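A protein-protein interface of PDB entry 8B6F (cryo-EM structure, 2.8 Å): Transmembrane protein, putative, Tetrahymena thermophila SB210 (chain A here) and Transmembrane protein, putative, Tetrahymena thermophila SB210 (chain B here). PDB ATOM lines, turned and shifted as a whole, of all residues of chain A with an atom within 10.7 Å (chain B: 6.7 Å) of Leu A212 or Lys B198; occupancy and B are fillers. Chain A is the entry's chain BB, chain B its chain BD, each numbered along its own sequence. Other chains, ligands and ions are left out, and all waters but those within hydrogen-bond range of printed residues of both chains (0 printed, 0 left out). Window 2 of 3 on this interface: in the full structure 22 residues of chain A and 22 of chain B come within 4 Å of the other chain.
The side-chain carboxylate (OE2) of Glu A208 is in salt-bridge range of the side-chain amino group (NZ) of Lys B199 (3.6 Å).
Among the printed residues, pairs that only touch across the chains: Leu A205 with Ile B195, Glu A208 with Ile B195, Leu A209 with Glu B194, Leu A209 with Ile B195, Leu A212 with Ile B195, Leu A212 with Lys B198 and Leu A212 with Lys B199.
Printed residues of chain B within 4 Å of Leu A205: Ile B195 (3.4 Å).
Glu A207 touches none of the printed residues of chain B.
Printed residues of chain B within 4 Å of Glu A208: Ile B195 and Lys B199.
Of the printed residues of chain B, Leu A209 touches Glu B194 and Ile B195.
Ala B193 touches none of the printed residues of chain A.
Of chain A, only Leu A209 (3.9 Å) comes within 4 Å of Glu B194.
Of the printed residues of chain A, Ile B195 touches Leu A205, Glu A208, Leu A209 and Leu A212.
No residue of chain A comes within 4 Å of Ala B196.
Of the printed residues of chain A, Lys B198 touches Leu A212 (3.6 Å).
Ala B201 touches none of the printed residues of chain A.
No residue of chain A comes within 4 Å of Ala B202.
The nearest residue of chain B that does not touch Leu A212 is Ala B202 (5.7 Å).
The nearest residue of chain A that does not touch Lys B198 is Leu A209 (4.5 Å).
The nearest printed residue of chain B that does not touch Leu A209 is Lys B198 (4.5 Å).
Of the 11 printed residues of chain A, 4 touch a printed residue of chain B.
Hydrophobic or aromatic side chains of chain A within 4 Å of the printed part of chain B: Leu A209 and Leu A212.
Among the printed residues, 8 pairs touch across the chains.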
ATOM      1  N   GLN A 204      22.385  -6.190  14.924  1.00  0.00           N
ATOM      2  CA  GLN A 204      22.141  -5.328  13.773  1.00  0.00           C
ATOM      3  C   GLN A 204      20.750  -5.559  13.199  1.00  0.00           C
ATOM      4  O   GLN A 204      20.033  -4.603  12.885  1.00  0.00           O
ATOM      5  CB  GLN A 204      23.207  -5.583  12.705  1.00  0.00           C
ATOM      6  CG  GLN A 204      23.016  -4.796  11.417  1.00  0.00           C
ATOM      7  CD  GLN A 204      23.976  -5.232  10.329  1.00  0.00           C
ATOM      8  OE1 GLN A 204      24.810  -6.112  10.537  1.00  0.00           O
ATOM      9  NE2 GLN A 204      23.858  -4.620   9.155  1.00  0.00           N
ATOM     10  N   LEU A 205      20.349  -6.823  13.057  1.00  0.00           N
ATOM     11  CA  LEU A 205      19.020  -7.119  12.532  1.00  0.00           C
ATOM     12  C   LEU A 205      17.931  -6.598  13.458  1.00  0.00           C
ATOM     13  O   LEU A 205      16.914  -6.068  12.996  1.00  0.00           O
ATOM     14  CB  LEU A 205      18.867  -8.623  12.317  1.00  0.00           C
ATOM     15  CG  LEU A 205      19.741  -9.232  11.218  1.00  0.00           C
ATOM     16  CD1 LEU A 205      19.504 -10.717  11.149  1.00  0.00           C
ATOM     17  CD2 LEU A 205      19.485  -8.594   9.862  1.00  0.00           C
ATOM     18  N   GLU A 206      18.121  -6.740  14.771  1.00  0.00           N
ATOM     19  CA  GLU A 206      17.132  -6.227  15.712  1.00  0.00           C
ATOM     20  C   GLU A 206      17.017  -4.713  15.610  1.00  0.00           C
ATOM     21  O   GLU A 206      15.911  -4.163  15.651  1.00  0.00           O
ATOM     22  CB  GLU A 206      17.491  -6.642  17.139  1.00  0.00           C
ATOM     23  CG  GLU A 206      17.203  -8.103  17.442  1.00  0.00           C
ATOM     24  CD  GLU A 206      17.392  -8.440  18.907  1.00  0.00           C
ATOM     25  OE1 GLU A 206      17.969  -7.608  19.638  1.00  0.00           O
ATOM     26  OE2 GLU A 206      16.959  -9.532  19.329  1.00  0.00           O
ATOM     27  N   GLU A 207      18.149  -4.020  15.479  1.00  0.00           N
ATOM     28  CA  GLU A 207      18.103  -2.571  15.317  1.00  0.00           C
ATOM     29  C   GLU A 207      17.379  -2.190  14.032  1.00  0.00           C
ATOM     30  O   GLU A 207      16.571  -1.254  14.020  1.00  0.00           O
ATOM     31  CB  GLU A 207      19.519  -1.998  15.323  1.00  0.00           C
ATOM     32  CG  GLU A 207      20.131  -1.870  16.707  1.00  0.00           C
ATOM     33  CD  GLU A 207      19.467  -0.788  17.539  1.00  0.00           C
ATOM     34  OE1 GLU A 207      18.509  -0.161  17.043  1.00  0.00           O
ATOM     35  OE2 GLU A 207      19.907  -0.563  18.685  1.00  0.00           O
ATOM     36  N   GLU A 208      17.652  -2.905  12.940  1.00  0.00           N
ATOM     37  CA  GLU A 208      16.958  -2.625  11.687  1.00  0.00           C
ATOM     38  C   GLU A 208      15.460  -2.850  11.833  1.00  0.00           C
ATOM     39  O   GLU A 208      14.653  -2.052  11.344  1.00  0.00           O
ATOM     40  CB  GLU A 208      17.524  -3.497  10.566  1.00  0.00           C
ATOM     41  CG  GLU A 208      16.890  -3.238   9.206  1.00  0.00           C
ATOM     42  CD  GLU A 208      17.447  -4.137   8.121  1.00  0.00           C
ATOM     43  OE1 GLU A 208      18.232  -5.050   8.447  1.00  0.00           O
ATOM     44  OE2 GLU A 208      17.099  -3.929   6.939  1.00  0.00           O
ATOM     45  N   LEU A 209      15.067  -3.936  12.503  1.00  0.00           N
ATOM     46  CA  LEU A 209      13.647  -4.205  12.699  1.00  0.00           C
ATOM     47  C   LEU A 209      12.992  -3.108  13.527  1.00  0.00           C
ATOM     48  O   LEU A 209      11.884  -2.661  13.214  1.00  0.00           O
ATOM     49  CB  LEU A 209      13.459  -5.567  13.368  1.00  0.00           C
ATOM     50  CG  LEU A 209      12.017  -5.991  13.670  1.00  0.00           C
ATOM     51  CD1 LEU A 209      11.218  -6.145  12.386  1.00  0.00           C
ATOM     52  CD2 LEU A 209      11.999  -7.283  14.468  1.00  0.00           C
ATOM     53  N   ALA A 210      13.663  -2.665  14.592  1.00  0.00           N
ATOM     54  CA  ALA A 210      13.108  -1.595  15.413  1.00  0.00           C
ATOM     55  C   ALA A 210      12.963  -0.309  14.612  1.00  0.00           C
ATOM     56  O   ALA A 210      11.941   0.379  14.705  1.00  0.00           O
ATOM     57  CB  ALA A 210      13.989  -1.366  16.641  1.00  0.00           C
ATOM     58  N   SER A 211      13.978   0.032  13.814  1.00  0.00           N
ATOM     59  CA  SER A 211      13.898   1.240  13.003  1.00  0.00           C
ATOM     60  C   SER A 211      12.756   1.151  12.000  1.00  0.00           C
ATOM     61  O   SER A 211      12.010   2.117  11.807  1.00  0.00           O
ATOM     62  CB  SER A 211      15.227   1.474  12.283  1.00  0.00           C
ATOM     63  OG  SER A 211      15.174   2.637  11.474  1.00  0.00           O
ATOM     64  N   LEU A 212      12.602  -0.006  11.354  1.00  0.00           N
ATOM     65  CA  LEU A 212      11.518  -0.175  10.391  1.00  0.00           C
ATOM     66  C   LEU A 212      10.161  -0.081  11.076  1.00  0.00           C
ATOM     67  O   LEU A 212       9.227   0.526  10.539  1.00  0.00           O
ATOM     68  CB  LEU A 212      11.663  -1.513   9.667  1.00  0.00           C
ATOM     69  CG  LEU A 212      10.670  -1.769   8.530  1.00  0.00           C
ATOM     70  CD1 LEU A 212      10.835  -0.741   7.419  1.00  0.00           C
ATOM     71  CD2 LEU A 212      10.835  -3.178   7.985  1.00  0.00           C
ATOM     72  N   ASN A 213      10.032  -0.680  12.261  1.00  0.00           N
ATOM     73  CA  ASN A 213       8.773  -0.602  12.994  1.00  0.00           C
ATOM     74  C   ASN A 213       8.448   0.835  13.375  1.00  0.00           C
ATOM     75  O   ASN A 213       7.290   1.261  13.290  1.00  0.00           O
ATOM     76  CB  ASN A 213       8.837  -1.486  14.240  1.00  0.00           C
ATOM     77  CG  ASN A 213       7.540  -1.482  15.024  1.00  0.00           C
ATOM     78  OD1 ASN A 213       6.499  -1.060  14.521  1.00  0.00           O
ATOM     79  ND2 ASN A 213       7.594  -1.958  16.263  1.00  0.00           N
ATOM     80  N   ASN A 214       9.451   1.596  13.803  1.00  0.00           N
ATOM     81  CA  ASN A 214       9.253   3.000  14.141  1.00  0.00           C
ATOM     82  C   ASN A 214       8.827   3.789  12.909  1.00  0.00           C
ATOM     83  O   ASN A 214       9.110   3.393  11.778  1.00  0.00           O
ATOM     84  CB  ASN A 214      10.528   3.601  14.732  1.00  0.00           C
ATOM     85  CG  ASN A 214      10.902   2.983  16.064  1.00  0.00           C
ATOM     86  OD1 ASN A 214      10.491   1.866  16.380  1.00  0.00           O
ATOM     87  ND2 ASN A 214      11.683   3.709  16.854  1.00  0.00           N
ATOM     88  OXT ASN A 214       8.195   4.840  13.014  1.00  0.00           O
ATOM     89  N   ALA B 193      13.240 -12.762   8.232  1.00  0.00           N
ATOM     90  CA  ALA B 193      11.920 -13.016   7.667  1.00  0.00           C
ATOM     91  C   ALA B 193      10.901 -12.006   8.179  1.00  0.00           C
ATOM     92  O   ALA B 193      10.055 -11.525   7.416  1.00  0.00           O
ATOM     93  CB  ALA B 193      11.473 -14.441   7.995  1.00  0.00           C
ATOM     94  N   GLU B 194      10.960 -11.677   9.472  1.00  0.00           N
ATOM     95  CA  GLU B 194      10.044 -10.682  10.019  1.00  0.00           C
ATOM     96  C   GLU B 194      10.269  -9.318   9.382  1.00  0.00           C
ATOM     97  O   GLU B 194       9.310  -8.608   9.062  1.00  0.00           O
ATOM     98  CB  GLU B 194      10.202 -10.602  11.537  1.00  0.00           C
ATOM     99  CG  GLU B 194       9.718 -11.844  12.266  1.00  0.00           C
ATOM    100  CD  GLU B 194       9.913 -11.754  13.766  1.00  0.00           C
ATOM    101  OE1 GLU B 194      10.022 -10.623  14.283  1.00  0.00           O
ATOM    102  OE2 GLU B 194       9.965 -12.813  14.427  1.00  0.00           O
ATOM    103  N   ILE B 195      11.532  -8.934   9.184  1.00  0.00           N
ATOM    104  CA  ILE B 195      11.820  -7.651   8.547  1.00  0.00           C
ATOM    105  C   ILE B 195      11.279  -7.640   7.125  1.00  0.00           C
ATOM    106  O   ILE B 195      10.689  -6.648   6.677  1.00  0.00           O
ATOM    107  CB  ILE B 195      13.333  -7.365   8.585  1.00  0.00           C
ATOM    108  CG1 ILE B 195      13.788  -7.131  10.027  1.00  0.00           C
ATOM    109  CG2 ILE B 195      13.677  -6.154   7.718  1.00  0.00           C
ATOM    110  CD1 ILE B 195      15.291  -7.050  10.197  1.00  0.00           C
ATOM    111  N   ALA B 196      11.471  -8.736   6.390  1.00  0.00           N
ATOM    112  CA  ALA B 196      10.953  -8.807   5.029  1.00  0.00           C
ATOM    113  C   ALA B 196       9.433  -8.715   5.018  1.00  0.00           C
ATOM    114  O   ALA B 196       8.850  -8.020   4.177  1.00  0.00           O
ATOM    115  CB  ALA B 196      11.417 -10.097   4.355  1.00  0.00           C
ATOM    116  N   ALA B 197       8.771  -9.406   5.948  1.00  0.00           N
ATOM    117  CA  ALA B 197       7.316  -9.337   6.018  1.00  0.00           C
ATOM    118  C   ALA B 197       6.849  -7.920   6.326  1.00  0.00           C
ATOM    119  O   ALA B 197       5.886  -7.432   5.725  1.00  0.00           O
ATOM    120  CB  ALA B 197       6.794 -10.315   7.071  1.00  0.00           C
ATOM    121  N   LYS B 198       7.522  -7.243   7.260  1.00  0.00           N
ATOM    122  CA  LYS B 198       7.162  -5.862   7.564  1.00  0.00           C
ATOM    123  C   LYS B 198       7.339  -4.969   6.345  1.00  0.00           C
ATOM    124  O   LYS B 198       6.483  -4.126   6.054  1.00  0.00           O
ATOM    125  CB  LYS B 198       8.003  -5.342   8.732  1.00  0.00           C
ATOM    126  CG  LYS B 198       7.326  -5.460  10.092  1.00  0.00           C
ATOM    127  CD  LYS B 198       7.223  -6.909  10.545  1.00  0.00           C
ATOM    128  CE  LYS B 198       6.522  -7.019  11.892  1.00  0.00           C
ATOM    129  NZ  LYS B 198       6.512  -8.420  12.401  1.00  0.00           N
ATOM    130  N   LYS B 199       8.445  -5.137   5.615  1.00  0.00           N
ATOM    131  CA  LYS B 199       8.668  -4.323   4.426  1.00  0.00           C
ATOM    132  C   LYS B 199       7.580  -4.557   3.386  1.00  0.00           C
ATOM    133  O   LYS B 199       7.051  -3.603   2.805  1.00  0.00           O
ATOM    134  CB  LYS B 199      10.045  -4.624   3.836  1.00  0.00           C
ATOM    135  CG  LYS B 199      11.205  -4.058   4.643  1.00  0.00           C
ATOM    136  CD  LYS B 199      12.532  -4.292   3.936  1.00  0.00           C
ATOM    137  CE  LYS B 199      13.688  -3.676   4.709  1.00  0.00           C
ATOM    138  NZ  LYS B 199      14.996  -3.916   4.036  1.00  0.00           N
ATOM    139  N   VAL B 200       7.227  -5.820   3.142  1.00  0.00           N
ATOM    140  CA  VAL B 200       6.207  -6.123   2.142  1.00  0.00           C
ATOM    141  C   VAL B 200       4.863  -5.545   2.565  1.00  0.00           C
ATOM    142  O   VAL B 200       4.138  -4.958   1.752  1.00  0.00           O
ATOM    143  CB  VAL B 200       6.126  -7.643   1.903  1.00  0.00           C
ATOM    144  CG1 VAL B 200       4.929  -7.996   1.025  1.00  0.00           C
ATOM    145  CG2 VAL B 200       7.411  -8.147   1.269  1.00  0.00           C
ATOM    146  N   ALA B 201       4.510  -5.698   3.842  1.00  0.00           N
ATOM    147  CA  ALA B 201       3.242  -5.159   4.323  1.00  0.00           C
ATOM    148  C   ALA B 201       3.210  -3.642   4.203  1.00  0.00           C
ATOM    149  O   ALA B 201       2.193  -3.064   3.805  1.00  0.00           O
ATOM    150  CB  ALA B 201       3.007  -5.587   5.771  1.00  0.00           C
ATOM    151  N   ALA B 202       4.316  -2.977   4.543  1.00  0.00           N
ATOM    152  CA  ALA B 202       4.360  -1.522   4.431  1.00  0.00           C
ATOM    153  C   ALA B 202       4.221  -1.078   2.981  1.00  0.00           C
ATOM    154  O   ALA B 202       3.501  -0.116   2.685  1.00  0.00           O
ATOM    155  CB  ALA B 202       5.660  -0.990   5.033  1.00  0.00           C
ATOM    156  N   LYS B 203       4.904  -1.762   2.061  1.00  0.00           N
ATOM    157  CA  LYS B 203       4.805  -1.397   0.651  1.00  0.00           C
ATOM    158  C   LYS B 203       3.393  -1.619   0.122  1.00  0.00           C
ATOM    159  O   LYS B 203       2.889  -0.818  -0.675  1.00  0.00           O
ATOM    160  CB  LYS B 203       5.819  -2.195  -0.170  1.00  0.00           C
ATOM    161  CG  LYS B 203       7.277  -1.879   0.158  1.00  0.00           C
ATOM    162  CD  LYS B 203       7.637  -0.439  -0.188  1.00  0.00           C
ATOM    163  CE  LYS B 203       9.096  -0.144   0.133  1.00  0.00           C
ATOM    164  NZ  LYS B 203       9.449   1.282  -0.131  1.00  0.00           N
